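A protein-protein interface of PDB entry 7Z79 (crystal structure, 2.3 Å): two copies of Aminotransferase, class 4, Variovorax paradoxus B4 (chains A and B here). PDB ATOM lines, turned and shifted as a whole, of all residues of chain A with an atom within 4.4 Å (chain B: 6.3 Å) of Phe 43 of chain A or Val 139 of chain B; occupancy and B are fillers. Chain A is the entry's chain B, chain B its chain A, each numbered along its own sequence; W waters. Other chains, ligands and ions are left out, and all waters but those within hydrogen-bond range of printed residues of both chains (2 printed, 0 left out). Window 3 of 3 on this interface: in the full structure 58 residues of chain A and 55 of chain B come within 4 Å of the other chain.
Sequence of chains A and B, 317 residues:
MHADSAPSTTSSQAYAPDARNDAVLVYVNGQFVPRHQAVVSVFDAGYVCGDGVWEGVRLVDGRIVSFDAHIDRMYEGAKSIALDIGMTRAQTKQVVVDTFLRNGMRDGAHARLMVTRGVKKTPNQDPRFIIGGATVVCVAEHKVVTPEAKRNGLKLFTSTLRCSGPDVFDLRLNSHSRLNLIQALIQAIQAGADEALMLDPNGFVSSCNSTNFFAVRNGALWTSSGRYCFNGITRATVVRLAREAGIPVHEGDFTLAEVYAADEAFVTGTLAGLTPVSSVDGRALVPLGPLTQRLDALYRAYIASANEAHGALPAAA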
ATOM      1  N   SER A  41     -21.429  -1.034 -25.641  1.00  0.00           N
ATOM      2  CA  SER A  41     -22.026  -2.042 -26.509  1.00  0.00           C
ATOM      3  C   SER A  41     -22.455  -3.282 -25.728  1.00  0.00           C
ATOM      4  O   SER A  41     -21.699  -3.736 -24.886  1.00  0.00           O
ATOM      5  CB  SER A  41     -21.085  -2.428 -27.658  1.00  0.00           C
ATOM      6  OG  SER A  41     -21.669  -3.487 -28.409  1.00  0.00           O
ATOM      7  N   VAL A  42     -23.615  -3.884 -26.097  1.00  0.00           N
ATOM      8  CA  VAL A  42     -23.998  -5.161 -25.491  1.00  0.00           C
ATOM      9  C   VAL A  42     -23.031  -6.266 -25.970  1.00  0.00           C
ATOM     10  O   VAL A  42     -23.128  -7.410 -25.544  1.00  0.00           O
ATOM     11  CB  VAL A  42     -25.471  -5.547 -25.798  1.00  0.00           C
ATOM     12  CG1 VAL A  42     -26.447  -4.452 -25.335  1.00  0.00           C
ATOM     13  CG2 VAL A  42     -25.728  -5.887 -27.288  1.00  0.00           C
ATOM     14  N   PHE A  43     -22.129  -5.956 -26.929  1.00  0.00           N
ATOM     15  CA  PHE A  43     -21.163  -6.918 -27.415  1.00  0.00           C
ATOM     16  C   PHE A  43     -19.835  -6.735 -26.676  1.00  0.00           C
ATOM     17  O   PHE A  43     -18.836  -7.336 -27.046  1.00  0.00           O
ATOM     18  CB  PHE A  43     -20.935  -6.740 -28.920  1.00  0.00           C
ATOM     19  CG  PHE A  43     -22.126  -7.109 -29.752  1.00  0.00           C
ATOM     20  CD1 PHE A  43     -23.165  -6.186 -29.959  1.00  0.00           C
ATOM     21  CD2 PHE A  43     -22.237  -8.386 -30.312  1.00  0.00           C
ATOM     22  CE1 PHE A  43     -24.264  -6.476 -30.771  1.00  0.00           C
ATOM     23  CE2 PHE A  43     -23.346  -8.728 -31.083  1.00  0.00           C
ATOM     24  CZ  PHE A  43     -24.353  -7.770 -31.328  1.00  0.00           C
ATOM     25  N   ASP A  44     -19.791  -5.805 -25.707  1.00  0.00           N
ATOM     26  CA  ASP A  44     -18.542  -5.584 -25.004  1.00  0.00           C
ATOM     27  C   ASP A  44     -18.195  -6.782 -24.127  1.00  0.00           C
ATOM     28  O   ASP A  44     -19.063  -7.347 -23.425  1.00  0.00           O
ATOM     29  CB  ASP A  44     -18.621  -4.332 -24.154  1.00  0.00           C
ATOM     30  CG  ASP A  44     -17.242  -3.938 -23.645  1.00  0.00           C
ATOM     31  OD1 ASP A  44     -16.846  -4.425 -22.560  1.00  0.00           O
ATOM     32  OD2 ASP A  44     -16.592  -3.150 -24.312  1.00  0.00           O
ATOM     33  N   ALA A  45     -16.904  -7.117 -24.102  1.00  0.00           N
ATOM     34  CA  ALA A  45     -16.436  -8.247 -23.303  1.00  0.00           C
ATOM     35  C   ALA A  45     -16.797  -8.095 -21.805  1.00  0.00           C
ATOM     36  O   ALA A  45     -17.067  -9.109 -21.093  1.00  0.00           O
ATOM     37  CB  ALA A  45     -14.951  -8.473 -23.538  1.00  0.00           C
ATOM     38  N   VAL A  48     -20.535  -8.960 -21.584  1.00  0.00           N
ATOM     39  CA  VAL A  48     -20.921 -10.316 -21.933  1.00  0.00           C
ATOM     40  C   VAL A  48     -20.374 -11.335 -20.931  1.00  0.00           C
ATOM     41  O   VAL A  48     -21.058 -12.316 -20.640  1.00  0.00           O
ATOM     42  CB  VAL A  48     -20.577 -10.695 -23.386  1.00  0.00           C
ATOM     43  CG1 VAL A  48     -20.947 -12.149 -23.714  1.00  0.00           C
ATOM     44  CG2 VAL A  48     -21.263  -9.711 -24.361  1.00  0.00           C
ATOM     45  N   GLY A 118     -12.984  -5.289 -24.807  1.00  0.00           N
ATOM     46  CA  GLY A 118     -13.385  -4.594 -26.021  1.00  0.00           C
ATOM     47  C   GLY A 118     -14.653  -5.163 -26.610  1.00  0.00           C
ATOM     48  O   GLY A 118     -15.270  -6.037 -25.996  1.00  0.00           O
ATOM     49  N   VAL A 119     -15.017  -4.614 -27.759  1.00  0.00           N
ATOM     50  CA  VAL A 119     -16.202  -5.029 -28.488  1.00  0.00           C
ATOM     51  C   VAL A 119     -15.963  -6.338 -29.254  1.00  0.00           C
ATOM     52  O   VAL A 119     -15.003  -6.489 -30.013  1.00  0.00           O
ATOM     53  CB  VAL A 119     -16.697  -3.879 -29.393  1.00  0.00           C
ATOM     54  CG1 VAL A 119     -17.955  -4.286 -30.146  1.00  0.00           C
ATOM     55  CG2 VAL A 119     -16.900  -2.568 -28.625  1.00  0.00           C
ATOM     56  N   LYS A 120     -16.872  -7.289 -29.053  1.00  0.00           N
ATOM     57  CA  LYS A 120     -16.725  -8.589 -29.703  1.00  0.00           C
ATOM     58  C   LYS A 120     -17.500  -8.647 -31.021  1.00  0.00           C
ATOM     59  O   LYS A 120     -18.538  -8.008 -31.130  1.00  0.00           O
ATOM     60  CB  LYS A 120     -17.237  -9.635 -28.721  1.00  0.00           C
ATOM     61  CG  LYS A 120     -16.291  -9.850 -27.544  1.00  0.00           C
ATOM     62  CD  LYS A 120     -16.924 -10.678 -26.448  1.00  0.00           C
ATOM     63  CE  LYS A 120     -15.882 -11.396 -25.611  1.00  0.00           C
ATOM     64  NZ  LYS A 120     -15.162 -12.460 -26.361  1.00  0.00           N
ATOM     65  N   PRO A 123     -21.135 -12.330 -29.245  1.00  0.00           N
ATOM     66  CA  PRO A 123     -21.024 -12.455 -27.791  1.00  0.00           C
ATOM     67  C   PRO A 123     -20.698 -13.914 -27.414  1.00  0.00           C
ATOM     68  O   PRO A 123     -21.477 -14.831 -27.666  1.00  0.00           O
ATOM     69  CB  PRO A 123     -22.409 -11.992 -27.323  1.00  0.00           C
ATOM     70  CG  PRO A 123     -23.336 -12.433 -28.444  1.00  0.00           C
ATOM     71  CD  PRO A 123     -22.523 -12.247 -29.694  1.00  0.00           C
ATOM     72  N   VAL B  24     -28.550  -6.985 -38.036  1.00  0.00           N
ATOM     73  CA  VAL B  24     -29.588  -7.560 -37.171  1.00  0.00           C
ATOM     74  C   VAL B  24     -29.996  -6.521 -36.112  1.00  0.00           C
ATOM     75  O   VAL B  24     -29.185  -5.663 -35.697  1.00  0.00           O
ATOM     76  CB  VAL B  24     -29.180  -8.907 -36.506  1.00  0.00           C
ATOM     77  CG1 VAL B  24     -28.882  -9.998 -37.523  1.00  0.00           C
ATOM     78  CG2 VAL B  24     -28.039  -8.760 -35.513  1.00  0.00           C
ATOM     79  N   LEU B  25     -31.250  -6.646 -35.680  1.00  0.00           N
ATOM     80  CA  LEU B  25     -31.774  -5.875 -34.562  1.00  0.00           C
ATOM     81  C   LEU B  25     -31.622  -6.691 -33.277  1.00  0.00           C
ATOM     82  O   LEU B  25     -31.900  -7.906 -33.284  1.00  0.00           O
ATOM     83  CB  LEU B  25     -33.226  -5.498 -34.837  1.00  0.00           C
ATOM     84  CG  LEU B  25     -33.451  -4.690 -36.125  1.00  0.00           C
ATOM     85  CD1 LEU B  25     -34.914  -4.693 -36.449  1.00  0.00           C
ATOM     86  CD2 LEU B  25     -33.123  -3.233 -35.892  1.00  0.00           C
ATOM     87  N   VAL B  26     -31.108  -6.015 -32.226  1.00  0.00           N
ATOM     88  CA  VAL B  26     -30.856  -6.613 -30.922  1.00  0.00           C
ATOM     89  C   VAL B  26     -31.954  -6.110 -30.013  1.00  0.00           C
ATOM     90  O   VAL B  26     -32.310  -4.920 -30.054  1.00  0.00           O
ATOM     91  CB  VAL B  26     -29.491  -6.151 -30.403  1.00  0.00           C
ATOM     92  CG1 VAL B  26     -29.207  -6.629 -28.976  1.00  0.00           C
ATOM     93  CG2 VAL B  26     -28.387  -6.542 -31.346  1.00  0.00           C
ATOM     94  N   TYR B  27     -32.518  -7.029 -29.240  1.00  0.00           N
ATOM     95  CA  TYR B  27     -33.469  -6.657 -28.191  1.00  0.00           C
ATOM     96  C   TYR B  27     -32.681  -6.103 -27.016  1.00  0.00           C
ATOM     97  O   TYR B  27     -31.754  -6.740 -26.521  1.00  0.00           O
ATOM     98  CB  TYR B  27     -34.262  -7.892 -27.801  1.00  0.00           C
ATOM     99  CG  TYR B  27     -35.319  -7.684 -26.749  1.00  0.00           C
ATOM    100  CD1 TYR B  27     -34.970  -7.646 -25.398  1.00  0.00           C
ATOM    101  CD2 TYR B  27     -36.666  -7.607 -27.113  1.00  0.00           C
ATOM    102  CE1 TYR B  27     -35.956  -7.485 -24.419  1.00  0.00           C
ATOM    103  CE2 TYR B  27     -37.663  -7.442 -26.144  1.00  0.00           C
ATOM    104  CZ  TYR B  27     -37.303  -7.388 -24.801  1.00  0.00           C
ATOM    105  OH  TYR B  27     -38.288  -7.287 -23.872  1.00  0.00           O
ATOM    106  N   ARG B  35     -27.745  -3.290 -34.417  1.00  0.00           N
ATOM    107  CA  ARG B  35     -26.516  -3.883 -33.894  1.00  0.00           C
ATOM    108  C   ARG B  35     -25.546  -2.829 -33.328  1.00  0.00           C
ATOM    109  O   ARG B  35     -25.160  -2.938 -32.177  1.00  0.00           O
ATOM    110  CB  ARG B  35     -25.942  -4.786 -34.993  1.00  0.00           C
ATOM    111  CG  ARG B  35     -24.747  -5.559 -34.511  1.00  0.00           C
ATOM    112  CD  ARG B  35     -23.878  -6.018 -35.699  1.00  0.00           C
ATOM    113  NE  ARG B  35     -22.848  -6.900 -35.078  1.00  0.00           N
ATOM    114  CZ  ARG B  35     -22.943  -8.207 -34.914  1.00  0.00           C
ATOM    115  NH1 ARG B  35     -24.001  -8.905 -35.329  1.00  0.00           N
ATOM    116  NH2 ARG B  35     -21.965  -8.790 -34.311  1.00  0.00           N
ATOM    117  N   HIS B  36     -25.189  -1.809 -34.133  1.00  0.00           N
ATOM    118  CA  HIS B  36     -24.115  -0.881 -33.802  1.00  0.00           C
ATOM    119  C   HIS B  36     -24.569   0.092 -32.727  1.00  0.00           C
ATOM    120  O   HIS B  36     -23.756   0.828 -32.190  1.00  0.00           O
ATOM    121  CB  HIS B  36     -23.531  -0.180 -35.062  1.00  0.00           C
ATOM    122  CG  HIS B  36     -22.911  -1.158 -36.007  1.00  0.00           C
ATOM    123  ND1 HIS B  36     -21.734  -1.933 -35.690  1.00  0.00           N
ATOM    124  CD2 HIS B  36     -23.356  -1.600 -37.213  1.00  0.00           C
ATOM    125  CE1 HIS B  36     -21.501  -2.769 -36.683  1.00  0.00           C
ATOM    126  NE2 HIS B  36     -22.488  -2.606 -37.620  1.00  0.00           N
ATOM    127  N   ALA B  38     -26.826  -1.061 -30.179  1.00  0.00           N
ATOM    128  CA  ALA B  38     -27.360  -1.860 -29.103  1.00  0.00           C
ATOM    129  C   ALA B  38     -26.393  -1.736 -27.935  1.00  0.00           C
ATOM    130  O   ALA B  38     -25.248  -2.170 -28.003  1.00  0.00           O
ATOM    131  CB  ALA B  38     -27.516  -3.285 -29.556  1.00  0.00           C
ATOM    132  N   THR B  99     -37.343 -11.642 -30.993  1.00  0.00           N
ATOM    133  CA  THR B  99     -36.045 -11.297 -31.542  1.00  0.00           C
ATOM    134  C   THR B  99     -35.814 -12.108 -32.833  1.00  0.00           C
ATOM    135  O   THR B  99     -35.324 -11.534 -33.817  1.00  0.00           O
ATOM    136  CB  THR B  99     -34.914 -11.447 -30.519  1.00  0.00           C
ATOM    137  OG1 THR B  99     -35.314 -10.723 -29.346  1.00  0.00           O
ATOM    138  CG2 THR B  99     -33.568 -10.948 -31.030  1.00  0.00           C
ATOM    139  N   HIS B 110     -29.122 -18.506 -34.056  1.00  0.00           N
ATOM    140  CA  HIS B 110     -28.737 -18.751 -32.685  1.00  0.00           C
ATOM    141  C   HIS B 110     -29.058 -17.432 -31.947  1.00  0.00           C
ATOM    142  O   HIS B 110     -28.861 -16.350 -32.506  1.00  0.00           O
ATOM    143  CB  HIS B 110     -27.237 -19.183 -32.641  1.00  0.00           C
ATOM    144  CG  HIS B 110     -26.608 -19.033 -31.285  1.00  0.00           C
ATOM    145  ND1 HIS B 110     -26.691 -20.066 -30.296  1.00  0.00           N
ATOM    146  CD2 HIS B 110     -25.973 -17.970 -30.669  1.00  0.00           C
ATOM    147  CE1 HIS B 110     -26.089 -19.671 -29.174  1.00  0.00           C
ATOM    148  NE2 HIS B 110     -25.700 -18.354 -29.363  1.00  0.00           N
ATOM    149  N   ALA B 111     -29.479 -17.514 -30.674  1.00  0.00           N
ATOM    150  CA  ALA B 111     -29.662 -16.288 -29.947  1.00  0.00           C
ATOM    151  C   ALA B 111     -29.020 -16.440 -28.584  1.00  0.00           C
ATOM    152  O   ALA B 111     -29.096 -17.513 -27.988  1.00  0.00           O
ATOM    153  CB  ALA B 111     -31.148 -15.930 -29.831  1.00  0.00           C
ATOM    154  N   ARG B 112     -28.446 -15.314 -28.108  1.00  0.00           N
ATOM    155  CA  ARG B 112     -27.985 -15.230 -26.753  1.00  0.00           C
ATOM    156  C   ARG B 112     -28.918 -14.308 -25.979  1.00  0.00           C
ATOM    157  O   ARG B 112     -29.047 -13.144 -26.292  1.00  0.00           O
ATOM    158  CB  ARG B 112     -26.513 -14.838 -26.703  1.00  0.00           C
ATOM    159  CG  ARG B 112     -25.899 -15.058 -25.320  1.00  0.00           C
ATOM    160  CD  ARG B 112     -24.537 -14.447 -25.344  1.00  0.00           C
ATOM    161  NE  ARG B 112     -23.721 -14.671 -24.185  1.00  0.00           N
ATOM    162  CZ  ARG B 112     -22.829 -15.650 -24.072  1.00  0.00           C
ATOM    163  NH1 ARG B 112     -22.657 -16.520 -25.045  1.00  0.00           N
ATOM    164  NH2 ARG B 112     -22.064 -15.762 -22.999  1.00  0.00           N
ATOM    165  N   LEU B 113     -29.624 -14.879 -25.001  1.00  0.00           N
ATOM    166  CA  LEU B 113     -30.499 -14.134 -24.105  1.00  0.00           C
ATOM    167  C   LEU B 113     -29.730 -13.866 -22.829  1.00  0.00           C
ATOM    168  O   LEU B 113     -29.317 -14.821 -22.148  1.00  0.00           O
ATOM    169  CB  LEU B 113     -31.782 -14.919 -23.835  1.00  0.00           C
ATOM    170  CG  LEU B 113     -32.716 -14.215 -22.839  1.00  0.00           C
ATOM    171  CD1 LEU B 113     -33.269 -12.925 -23.420  1.00  0.00           C
ATOM    172  CD2 LEU B 113     -33.819 -15.139 -22.348  1.00  0.00           C
ATOM    173  N   MET B 114     -29.495 -12.570 -22.568  1.00  0.00           N
ATOM    174  CA  MET B 114     -28.705 -12.107 -21.441  1.00  0.00           C
ATOM    175  C   MET B 114     -29.582 -11.275 -20.493  1.00  0.00           C
ATOM    176  O   MET B 114     -30.259 -10.360 -20.933  1.00  0.00           O
ATOM    177  CB  MET B 114     -27.538 -11.269 -21.967  1.00  0.00           C
ATOM    178  CG  MET B 114     -26.530 -12.129 -22.685  1.00  0.00           C
ATOM    179  SD  MET B 114     -25.199 -11.157 -23.380  1.00  0.00           S
ATOM    180  CE  MET B 114     -25.956 -10.340 -24.806  1.00  0.00           C
ATOM    181  N   VAL B 137     -31.289  -8.432 -22.708  1.00  0.00           N
ATOM    182  CA  VAL B 137     -30.711  -8.300 -24.036  1.00  0.00           C
ATOM    183  C   VAL B 137     -30.798  -9.625 -24.756  1.00  0.00           C
ATOM    184  O   VAL B 137     -30.552 -10.670 -24.167  1.00  0.00           O
ATOM    185  CB  VAL B 137     -29.256  -7.843 -23.947  1.00  0.00           C
ATOM    186  CG1 VAL B 137     -28.604  -7.767 -25.336  1.00  0.00           C
ATOM    187  CG2 VAL B 137     -29.156  -6.498 -23.230  1.00  0.00           C
ATOM    188  N   CYS B 138     -31.165  -9.562 -26.026  1.00  0.00           N
ATOM    189  CA  CYS B 138     -31.227 -10.740 -26.865  1.00  0.00           C
ATOM    190  C   CYS B 138     -30.562 -10.453 -28.200  1.00  0.00           C
ATOM    191  O   CYS B 138     -31.012  -9.604 -28.953  1.00  0.00           O
ATOM    192  CB  CYS B 138     -32.649 -11.204 -27.071  1.00  0.00           C
ATOM    193  SG  CYS B 138     -32.645 -12.893 -27.742  1.00  0.00           S
ATOM    194  N   VAL B 139     -29.457 -11.146 -28.450  1.00  0.00           N
ATOM    195  CA  VAL B 139     -28.675 -11.006 -29.679  1.00  0.00           C
ATOM    196  C   VAL B 139     -28.939 -12.258 -30.504  1.00  0.00           C
ATOM    197  O   VAL B 139     -28.485 -13.331 -30.129  1.00  0.00           O
ATOM    198  CB  VAL B 139     -27.154 -10.884 -29.427  1.00  0.00           C
ATOM    199  CG1 VAL B 139     -26.452 -10.714 -30.755  1.00  0.00           C
ATOM    200  CG2 VAL B 139     -26.839  -9.641 -28.596  1.00  0.00           C
ATOM    201  N   ALA B 140     -29.670 -12.097 -31.611  1.00  0.00           N
ATOM    202  CA  ALA B 140     -29.893 -13.198 -32.547  1.00  0.00           C
ATOM    203  C   ALA B 140     -29.015 -12.965 -33.770  1.00  0.00           C
ATOM    204  O   ALA B 140     -28.877 -11.846 -34.201  1.00  0.00           O
ATOM    205  CB  ALA B 140     -31.331 -13.299 -32.932  1.00  0.00           C
ATOM    206  N   GLU B 141     -28.385 -14.035 -34.242  1.00  0.00           N
ATOM    207  CA  GLU B 141     -27.457 -13.955 -35.390  1.00  0.00           C
ATOM    208  C   GLU B 141     -27.563 -15.217 -36.243  1.00  0.00           C
ATOM    209  O   GLU B 141     -27.815 -16.268 -35.671  1.00  0.00           O
ATOM    210  CB  GLU B 141     -26.021 -13.813 -34.894  1.00  0.00           C
ATOM    211  CG  GLU B 141     -25.544 -12.391 -34.701  1.00  0.00           C
ATOM    212  CD  GLU B 141     -24.151 -12.329 -34.104  1.00  0.00           C
ATOM    213  OE1 GLU B 141     -23.941 -12.950 -33.052  1.00  0.00           O
ATOM    214  OE2 GLU B 141     -23.281 -11.681 -34.705  1.00  0.00           O
HETATM  215  O   HOH W   1     -23.425  -2.285 -29.968  1.00  0.00           O
HETATM  216  O   HOH W   2     -23.268 -13.658 -21.565  1.00  0.00           O
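Printed residues of chain B within 4 Å of Ser 41 of chain A: Ala 38 (3.6 Å).
Of chain B, only Arg 35 (3.5 Å) and Val 139 (3.7 Å) come within 4 Å of Phe 43 of chain A.
Printed residues of chain B within 4 Å of Val 48 of chain A: Arg 112.
Of the printed residues of chain A, Arg 35 of chain B touches Phe 43 (3.5 Å).
His 110 of chain B touches none of the printed residues of chain A.
Of the printed residues of chain A, Val 137 of chain B touches Val 42.
Cys 138 of chain B touches none of the printed residues of chain A.
Printed residues of chain A within 4 Å of Glu 141 of chain B: Pro 123.
The nearest residue of chain B that does not touch Phe 43 of chain A is Val 26 of chain B (4.2 Å).
No position is printed for both chains.
The backbone NH of Val 42 of chain A sits at hydrogen-bond distance from the backbone carbonyl oxygen of Ala 38 of chain B.
The guanidinium group (NH1) of Arg 112 of chain B sits at hydrogen-bond distance from the backbone carbonyl oxygen (O) of Pro 123 of chain A.
CA of Ser 41 of chain A touches O of Ala 38 of chain B, 3.6 Å away.
Val 42 of chain A touches Val 26 of chain B (CG2 to CG1, 3.9 Å).
CB of Val 42 of chain A touches CG1 of Val 137 of chain B (3.9 Å).
Arg 35 of chain B touches Phe 43 of chain A (NH2 to CE2, 3.5 Å).
Val 139 of chain B touches Phe 43 of chain A (CG1 to CZ, 3.7 Å).
Arg 112 of chain B touches Val 48 of chain A (NE to CG1, 3.8 Å).
OE1 of Glu 141 of chain B touches CD of Pro 123 of chain A, 3.7 Å away.
Water W1 lies within hydrogen-bond range of the side-chain hydroxyl of Ser 41 of chain A (2.6 Å), the backbone carbonyl oxygen of Ala 38 of chain B (2.7 Å) and the backbone carbonyl oxygen of Arg 35 of chain B (2.9 Å).
Water W2 lies within hydrogen-bond range of O of Val 48 of chain A (2.7 Å), NH2 of Arg 112 of chain B (2.8 Å) and SD of Met 114 of chain B (3.6 Å).
The guanidinium group (NH1) of Arg 35 of chain B is in salt-bridge range of the side-chain carboxylate (OE2) of Glu 141 of chain B (2.9 Å).
The backbone carbonyl oxygen (O) of His 110 of chain B sits at hydrogen-bond distance from the backbone NH (N) of Glu 141 of chain B.
N of Phe 43 of chain A lies within hydrogen-bond range of OG of Ser 41 of chain A (2.9 Å).
The backbone NH of Arg 112 of chain B sits at hydrogen-bond distance from the backbone carbonyl oxygen of Val 139 of chain B, at 2.8 Å.
The backbone NH of Lys 120 of chain A is in hydrogen-bond range of the backbone carbonyl oxygen of Phe 43 of chain A (2.8 Å).
N of Met 114 of chain B sits at hydrogen-bond distance from O of Val 137 of chain B, at 2.7 Å.
Of the 18 printed residues of chain B, 7 touch a printed residue of chain A.
Hydrophobic or aromatic side chains of chain B that line the printed part of chain A: Val 26, Ala 38, Val 137 and Val 139.
Printed residues of chain A that touch a printed residue of chain B: Ser 41, Val 42, Phe 43, Val 48 and Pro 123.
Among the printed residues, 9 pairs touch across the chains.
Among the printed residues, no Asp or Glu carboxylate lies within 4 Å of a Lys or Arg side-chain nitrogen of the other chain.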
